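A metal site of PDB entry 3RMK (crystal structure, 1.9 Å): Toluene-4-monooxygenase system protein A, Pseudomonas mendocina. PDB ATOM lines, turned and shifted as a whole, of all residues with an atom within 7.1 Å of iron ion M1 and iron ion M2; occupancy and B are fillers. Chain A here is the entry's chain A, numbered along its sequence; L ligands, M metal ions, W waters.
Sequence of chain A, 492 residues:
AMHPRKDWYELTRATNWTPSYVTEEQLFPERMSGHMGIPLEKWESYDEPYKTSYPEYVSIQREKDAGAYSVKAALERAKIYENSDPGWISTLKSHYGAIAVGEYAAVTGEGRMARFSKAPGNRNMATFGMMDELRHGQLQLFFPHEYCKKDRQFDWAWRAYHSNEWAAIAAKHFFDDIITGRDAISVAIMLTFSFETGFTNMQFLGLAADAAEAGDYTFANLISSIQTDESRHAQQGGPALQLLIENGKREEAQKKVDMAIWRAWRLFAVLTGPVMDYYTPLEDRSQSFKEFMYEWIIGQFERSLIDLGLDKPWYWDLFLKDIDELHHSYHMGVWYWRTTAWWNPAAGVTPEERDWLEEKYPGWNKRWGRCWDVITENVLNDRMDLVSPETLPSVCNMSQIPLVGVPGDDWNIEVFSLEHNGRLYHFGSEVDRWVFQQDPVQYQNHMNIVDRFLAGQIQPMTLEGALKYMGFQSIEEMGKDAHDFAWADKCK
Iron ion M1 is bound by water W2, OE1 of Glu 103, OE1 of Glu 133, water W1 and ND1 of His 136.
Iron ion M1 has five donor atoms within binding distance.
Slightly farther from iron ion M1 lies an oxygen (O1) of the ligand (2.7 Å).
The nearest printed residue that does not touch iron ion M1 is His 233 (4.5 Å).
Water W1 bridges the side-chain carboxylate (OE2) of Glu 103 (2.6 Å) and the side-chain carboxylate (OE1) of Glu 230 (3.3 Å).
The backbone carbonyl oxygen (O) of Glu 196 sits at hydrogen-bond distance from the side-chain hydroxyl (OG1) of Thr 200.
The backbone NH (N) of Glu 196 is in hydrogen-bond range of the backbone carbonyl oxygen (O) of Leu 191, at 2.9 Å.
OE2 of Glu 103 is in hydrogen-bond range of NE2 of Gln 140, 3.0 Å away.
A ring nitrogen (ND1) of His 233 lies within hydrogen-bond range of the side-chain carboxylate of Asp 132.
ND1 of His 136 sits close to O of Asp 132, at 3.5 Å.
O of His 136 lies within hydrogen-bond range of NE2 of Gln 140 (3.1 Å).
OD2 of Asp 229 sits at hydrogen-bond distance from NE2 of His 136, 2.5 Å away.
Of the 23 residues printed, 4 come within 4 Å of iron ion M2.
The nearest printed residue that does not touch iron ion M2 is His 136 (4.7 Å).
OE2 of Glu 196 binds iron ion M2 (1.9 Å).
O1 of the ligand is bound to iron ion M2.
Water W2 binds iron ion M2, 2.0 Å away.
OE2 of Glu 133 binds iron ion M2 (2.0 Å).
NE2 of His 233 binds iron ion M2, at 2.1 Å.
OE2 of Glu 230 binds iron ion M2.
Iron ion M2 has six donor atoms within binding distance.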
ATOM      1  N   ILE A  99       8.950  -7.832  -2.069  1.00  0.00           N
ATOM      2  CA  ILE A  99       9.622  -6.734  -1.371  1.00  0.00           C
ATOM      3  C   ILE A  99       8.919  -6.159  -0.137  1.00  0.00           C
ATOM      4  O   ILE A  99       9.586  -5.804   0.841  1.00  0.00           O
ATOM      5  CB  ILE A  99       9.921  -5.566  -2.338  1.00  0.00           C
ATOM      6  CG1 ILE A  99      10.899  -6.018  -3.435  1.00  0.00           C
ATOM      7  CG2 ILE A  99      10.491  -4.369  -1.572  1.00  0.00           C
ATOM      8  CD1 ILE A  99      12.225  -6.561  -2.877  1.00  0.00           C
ATOM      9  N   GLU A 103      10.780  -5.430   3.310  1.00  0.00           N
ATOM     10  CA  GLU A 103      11.153  -4.104   3.818  1.00  0.00           C
ATOM     11  C   GLU A 103      10.842  -4.056   5.309  1.00  0.00           C
ATOM     12  O   GLU A 103      11.657  -3.585   6.093  1.00  0.00           O
ATOM     13  CB  GLU A 103      10.401  -2.974   3.122  1.00  0.00           C
ATOM     14  CG  GLU A 103      10.686  -2.830   1.622  1.00  0.00           C
ATOM     15  CD  GLU A 103      11.699  -1.746   1.305  1.00  0.00           C
ATOM     16  OE1 GLU A 103      12.421  -1.303   2.232  1.00  0.00           O
ATOM     17  OE2 GLU A 103      11.749  -1.334   0.126  1.00  0.00           O
ATOM     18  N   ALA A 106      13.308  -5.812   7.331  1.00  0.00           N
ATOM     19  CA  ALA A 106      14.556  -5.055   7.474  1.00  0.00           C
ATOM     20  C   ALA A 106      14.534  -4.117   8.695  1.00  0.00           C
ATOM     21  O   ALA A 106      15.589  -3.731   9.202  1.00  0.00           O
ATOM     22  CB  ALA A 106      14.887  -4.272   6.195  1.00  0.00           C
ATOM     23  N   GLU A 110      17.805  -3.657  11.221  1.00  0.00           N
ATOM     24  CA  GLU A 110      18.196  -2.348  11.753  1.00  0.00           C
ATOM     25  C   GLU A 110      18.122  -2.316  13.285  1.00  0.00           C
ATOM     26  O   GLU A 110      19.037  -1.836  13.932  1.00  0.00           O
ATOM     27  CB  GLU A 110      17.355  -1.249  11.115  1.00  0.00           C
ATOM     28  CG  GLU A 110      17.563  -1.143   9.576  1.00  0.00           C
ATOM     29  CD  GLU A 110      18.890  -0.468   9.199  1.00  0.00           C
ATOM     30  OE1 GLU A 110      19.532   0.102  10.085  1.00  0.00           O
ATOM     31  OE2 GLU A 110      19.288  -0.499   8.009  1.00  0.00           O
ATOM     32  N   GLY A 129      17.375   3.886  10.405  1.00  0.00           N
ATOM     33  CA  GLY A 129      17.135   2.739   9.513  1.00  0.00           C
ATOM     34  C   GLY A 129      15.847   1.996   9.833  1.00  0.00           C
ATOM     35  O   GLY A 129      15.108   1.593   8.937  1.00  0.00           O
ATOM     36  N   ASP A 132      13.178   4.229   8.493  1.00  0.00           N
ATOM     37  CA  ASP A 132      13.156   4.176   7.037  1.00  0.00           C
ATOM     38  C   ASP A 132      12.459   2.916   6.559  1.00  0.00           C
ATOM     39  O   ASP A 132      11.624   2.966   5.651  1.00  0.00           O
ATOM     40  CB  ASP A 132      14.576   4.188   6.445  1.00  0.00           C
ATOM     41  CG  ASP A 132      15.225   5.547   6.521  1.00  0.00           C
ATOM     42  OD1 ASP A 132      14.528   6.556   6.801  1.00  0.00           O
ATOM     43  OD2 ASP A 132      16.451   5.608   6.287  1.00  0.00           O
ATOM     44  N   GLU A 133      12.828   1.788   7.135  1.00  0.00           N
ATOM     45  CA  GLU A 133      12.305   0.522   6.621  1.00  0.00           C
ATOM     46  C   GLU A 133      10.835   0.382   7.019  1.00  0.00           C
ATOM     47  O   GLU A 133      10.045  -0.227   6.299  1.00  0.00           O
ATOM     48  CB  GLU A 133      13.159  -0.668   7.064  1.00  0.00           C
ATOM     49  CG  GLU A 133      14.649  -0.594   6.621  1.00  0.00           C
ATOM     50  CD  GLU A 133      14.851  -0.473   5.090  1.00  0.00           C
ATOM     51  OE1 GLU A 133      13.877  -0.256   4.340  1.00  0.00           O
ATOM     52  OE2 GLU A 133      16.006  -0.574   4.645  1.00  0.00           O
ATOM     53  N   LEU A 134      10.479   0.989   8.152  1.00  0.00           N
ATOM     54  CA  LEU A 134       9.075   1.036   8.539  1.00  0.00           C
ATOM     55  C   LEU A 134       8.279   1.808   7.492  1.00  0.00           C
ATOM     56  O   LEU A 134       7.182   1.399   7.097  1.00  0.00           O
ATOM     57  CB  LEU A 134       8.901   1.714   9.896  1.00  0.00           C
ATOM     58  CG  LEU A 134       7.431   1.887  10.303  1.00  0.00           C
ATOM     59  CD1 LEU A 134       6.766   0.521  10.511  1.00  0.00           C
ATOM     60  CD2 LEU A 134       7.312   2.737  11.571  1.00  0.00           C
ATOM     61  N   ARG A 135       8.818   2.941   7.054  1.00  0.00           N
ATOM     62  CA  ARG A 135       8.173   3.728   6.010  1.00  0.00           C
ATOM     63  C   ARG A 135       7.990   2.885   4.747  1.00  0.00           C
ATOM     64  O   ARG A 135       6.942   2.901   4.111  1.00  0.00           O
ATOM     65  CB  ARG A 135       9.016   4.953   5.650  1.00  0.00           C
ATOM     66  CG  ARG A 135       8.353   5.829   4.567  1.00  0.00           C
ATOM     67  CD  ARG A 135       9.282   6.897   3.980  1.00  0.00           C
ATOM     68  NE  ARG A 135       8.507   7.714   3.065  1.00  0.00           N
ATOM     69  CZ  ARG A 135       8.908   8.148   1.874  1.00  0.00           C
ATOM     70  NH1 ARG A 135      10.136   7.906   1.434  1.00  0.00           N
ATOM     71  NH2 ARG A 135       8.059   8.856   1.137  1.00  0.00           N
ATOM     72  N   HIS A 136       9.051   2.171   4.369  1.00  0.00           N
ATOM     73  CA  HIS A 136       9.035   1.472   3.082  1.00  0.00           C
ATOM     74  C   HIS A 136       8.094   0.303   3.117  1.00  0.00           C
ATOM     75  O   HIS A 136       7.459  -0.007   2.108  1.00  0.00           O
ATOM     76  CB  HIS A 136      10.464   1.060   2.658  1.00  0.00           C
ATOM     77  CG  HIS A 136      11.398   2.221   2.541  1.00  0.00           C
ATOM     78  ND1 HIS A 136      12.766   2.089   2.479  1.00  0.00           N
ATOM     79  CD2 HIS A 136      11.147   3.558   2.526  1.00  0.00           C
ATOM     80  CE1 HIS A 136      13.325   3.281   2.403  1.00  0.00           C
ATOM     81  NE2 HIS A 136      12.364   4.189   2.440  1.00  0.00           N
ATOM     82  N   GLY A 137       7.977  -0.331   4.277  1.00  0.00           N
ATOM     83  CA  GLY A 137       7.055  -1.434   4.468  1.00  0.00           C
ATOM     84  C   GLY A 137       5.607  -0.983   4.411  1.00  0.00           C
ATOM     85  O   GLY A 137       4.753  -1.621   3.798  1.00  0.00           O
ATOM     86  N   GLN A 140       4.579   0.277   0.824  1.00  0.00           N
ATOM     87  CA  GLN A 140       4.447  -0.810  -0.149  1.00  0.00           C
ATOM     88  C   GLN A 140       3.398  -1.853   0.246  1.00  0.00           C
ATOM     89  O   GLN A 140       3.216  -2.853  -0.427  1.00  0.00           O
ATOM     90  CB  GLN A 140       5.824  -1.420  -0.464  1.00  0.00           C
ATOM     91  CG  GLN A 140       6.638  -0.469  -1.345  1.00  0.00           C
ATOM     92  CD  GLN A 140       8.097  -0.861  -1.557  1.00  0.00           C
ATOM     93  OE1 GLN A 140       8.509  -1.177  -2.672  1.00  0.00           O
ATOM     94  NE2 GLN A 140       8.880  -0.768  -0.486  1.00  0.00           N
ATOM     95  N   LEU A 191      23.478  -6.918   4.722  1.00  0.00           N
ATOM     96  CA  LEU A 191      22.333  -6.113   4.310  1.00  0.00           C
ATOM     97  C   LEU A 191      22.738  -4.744   3.759  1.00  0.00           C
ATOM     98  O   LEU A 191      22.546  -4.481   2.597  1.00  0.00           O
ATOM     99  CB  LEU A 191      21.311  -5.956   5.442  1.00  0.00           C
ATOM    100  CG  LEU A 191      20.170  -4.955   5.165  1.00  0.00           C
ATOM    101  CD1 LEU A 191      19.280  -5.384   3.983  1.00  0.00           C
ATOM    102  CD2 LEU A 191      19.328  -4.744   6.420  1.00  0.00           C
ATOM    103  N   THR A 192      23.298  -3.875   4.587  1.00  0.00           N
ATOM    104  CA  THR A 192      23.461  -2.471   4.181  1.00  0.00           C
ATOM    105  C   THR A 192      24.538  -2.279   3.102  1.00  0.00           C
ATOM    106  O   THR A 192      24.307  -1.558   2.151  1.00  0.00           O
ATOM    107  CB  THR A 192      23.625  -1.497   5.370  1.00  0.00           C
ATOM    108  OG1 THR A 192      24.950  -1.582   5.909  1.00  0.00           O
ATOM    109  CG2 THR A 192      22.603  -1.827   6.477  1.00  0.00           C
ATOM    110  N   GLU A 196      21.848  -3.612  -0.031  1.00  0.00           N
ATOM    111  CA  GLU A 196      21.257  -2.288  -0.231  1.00  0.00           C
ATOM    112  C   GLU A 196      22.113  -1.375  -1.095  1.00  0.00           C
ATOM    113  O   GLU A 196      21.669  -0.894  -2.131  1.00  0.00           O
ATOM    114  CB  GLU A 196      20.944  -1.618   1.120  1.00  0.00           C
ATOM    115  CG  GLU A 196      19.782  -2.332   1.826  1.00  0.00           C
ATOM    116  CD  GLU A 196      19.414  -1.706   3.169  1.00  0.00           C
ATOM    117  OE1 GLU A 196      20.297  -1.549   4.019  1.00  0.00           O
ATOM    118  OE2 GLU A 196      18.234  -1.393   3.373  1.00  0.00           O
ATOM    119  N   THR A 200      20.077  -2.908  -4.342  1.00  0.00           N
ATOM    120  CA  THR A 200      18.765  -2.255  -4.352  1.00  0.00           C
ATOM    121  C   THR A 200      18.831  -0.787  -4.774  1.00  0.00           C
ATOM    122  O   THR A 200      17.912  -0.274  -5.379  1.00  0.00           O
ATOM    123  CB  THR A 200      18.029  -2.378  -2.999  1.00  0.00           C
ATOM    124  OG1 THR A 200      18.773  -1.701  -1.996  1.00  0.00           O
ATOM    125  CG2 THR A 200      17.889  -3.844  -2.597  1.00  0.00           C
ATOM    126  N   PHE A 204      16.324   0.166  -7.658  1.00  0.00           N
ATOM    127  CA  PHE A 204      15.201   1.099  -7.475  1.00  0.00           C
ATOM    128  C   PHE A 204      15.259   2.271  -8.458  1.00  0.00           C
ATOM    129  O   PHE A 204      14.248   2.675  -9.009  1.00  0.00           O
ATOM    130  CB  PHE A 204      15.083   1.557  -6.018  1.00  0.00           C
ATOM    131  CG  PHE A 204      14.306   0.588  -5.126  1.00  0.00           C
ATOM    132  CD1 PHE A 204      14.456  -0.778  -5.257  1.00  0.00           C
ATOM    133  CD2 PHE A 204      13.419   1.061  -4.169  1.00  0.00           C
ATOM    134  CE1 PHE A 204      13.737  -1.680  -4.440  1.00  0.00           C
ATOM    135  CE2 PHE A 204      12.698   0.186  -3.341  1.00  0.00           C
ATOM    136  CZ  PHE A 204      12.854  -1.189  -3.490  1.00  0.00           C
ATOM    137  N   ILE A 226      11.262   6.360  -2.157  1.00  0.00           N
ATOM    138  CA  ILE A 226      11.906   5.335  -1.352  1.00  0.00           C
ATOM    139  C   ILE A 226      13.416   5.288  -1.552  1.00  0.00           C
ATOM    140  O   ILE A 226      14.185   5.177  -0.590  1.00  0.00           O
ATOM    141  CB  ILE A 226      11.290   3.957  -1.651  1.00  0.00           C
ATOM    142  CG1 ILE A 226       9.850   3.925  -1.125  1.00  0.00           C
ATOM    143  CG2 ILE A 226      12.196   2.848  -1.106  1.00  0.00           C
ATOM    144  CD1 ILE A 226       9.044   2.663  -1.487  1.00  0.00           C
ATOM    145  N   ASP A 229      15.744   7.574   0.422  1.00  0.00           N
ATOM    146  CA  ASP A 229      16.024   7.209   1.809  1.00  0.00           C
ATOM    147  C   ASP A 229      17.231   6.287   1.940  1.00  0.00           C
ATOM    148  O   ASP A 229      17.814   6.160   3.013  1.00  0.00           O
ATOM    149  CB  ASP A 229      14.840   6.441   2.420  1.00  0.00           C
ATOM    150  CG  ASP A 229      13.607   7.281   2.600  1.00  0.00           C
ATOM    151  OD1 ASP A 229      13.734   8.504   2.841  1.00  0.00           O
ATOM    152  OD2 ASP A 229      12.502   6.706   2.542  1.00  0.00           O
ATOM    153  N   GLU A 230      17.592   5.618   0.849  1.00  0.00           N
ATOM    154  CA  GLU A 230      18.475   4.457   0.934  1.00  0.00           C
ATOM    155  C   GLU A 230      19.812   4.734   1.614  1.00  0.00           C
ATOM    156  O   GLU A 230      20.205   4.006   2.518  1.00  0.00           O
ATOM    157  CB  GLU A 230      18.704   3.791  -0.437  1.00  0.00           C
ATOM    158  CG  GLU A 230      19.074   2.305  -0.326  1.00  0.00           C
ATOM    159  CD  GLU A 230      17.975   1.489   0.362  1.00  0.00           C
ATOM    160  OE1 GLU A 230      16.781   1.720   0.061  1.00  0.00           O
ATOM    161  OE2 GLU A 230      18.295   0.628   1.218  1.00  0.00           O
ATOM    162  N   SER A 231      20.514   5.780   1.179  1.00  0.00           N
ATOM    163  CA  SER A 231      21.886   6.014   1.632  1.00  0.00           C
ATOM    164  C   SER A 231      21.955   6.284   3.134  1.00  0.00           C
ATOM    165  O   SER A 231      22.979   6.005   3.790  1.00  0.00           O
ATOM    166  CB  SER A 231      22.536   7.163   0.860  1.00  0.00           C
ATOM    167  OG  SER A 231      22.035   8.408   1.314  1.00  0.00           O
ATOM    168  N   HIS A 233      20.687   4.804   5.633  1.00  0.00           N
ATOM    169  CA  HIS A 233      20.964   3.601   6.432  1.00  0.00           C
ATOM    170  C   HIS A 233      21.845   2.602   5.712  1.00  0.00           C
ATOM    171  O   HIS A 233      22.517   1.780   6.346  1.00  0.00           O
ATOM    172  CB  HIS A 233      19.655   2.934   6.900  1.00  0.00           C
ATOM    173  CG  HIS A 233      18.774   2.490   5.774  1.00  0.00           C
ATOM    174  ND1 HIS A 233      17.730   3.257   5.306  1.00  0.00           N
ATOM    175  CD2 HIS A 233      18.825   1.384   4.992  1.00  0.00           C
ATOM    176  CE1 HIS A 233      17.154   2.620   4.293  1.00  0.00           C
ATOM    177  NE2 HIS A 233      17.797   1.488   4.086  1.00  0.00           N
ATOM    178  N   ALA A 234      21.860   2.651   4.375  1.00  0.00           N
ATOM    179  CA  ALA A 234      22.674   1.713   3.623  1.00  0.00           C
ATOM    180  C   ALA A 234      24.161   2.035   3.813  1.00  0.00           C
ATOM    181  O   ALA A 234      25.011   1.181   3.583  1.00  0.00           O
ATOM    182  CB  ALA A 234      22.299   1.748   2.120  1.00  0.00           C
HETATM  183  O1  LIG L   1      16.054  -1.364   1.783  1.00  0.00           O
HETATM  184  C1  LIG L   1      15.540  -2.604   1.623  1.00  0.00           C
HETATM  185  C2  LIG L   1      15.544  -3.482   2.697  1.00  0.00           C
HETATM  186  C3  LIG L   1      15.012  -4.746   2.548  1.00  0.00           C
HETATM  187  C4  LIG L   1      14.479  -5.125   1.321  1.00  0.00           C
HETATM  188  C5  LIG L   1      14.475  -4.248   0.247  1.00  0.00           C
HETATM  189  C6  LIG L   1      15.018  -2.982   0.405  1.00  0.00           C
HETATM  190 BR1  LIG L   1      13.755  -6.853   1.128  1.00  0.00          BR
HETATM  191 FE    FE M   1      13.874   0.100   2.246  1.00  0.00          FE
HETATM  192 FE    FE M   2      16.938  -0.033   2.912  1.00  0.00          FE
HETATM  193  O   HOH W   1      13.856   0.102   0.085  1.00  0.00           O
HETATM  194  O   HOH W   2      15.484   1.067   2.161  1.00  0.00           O
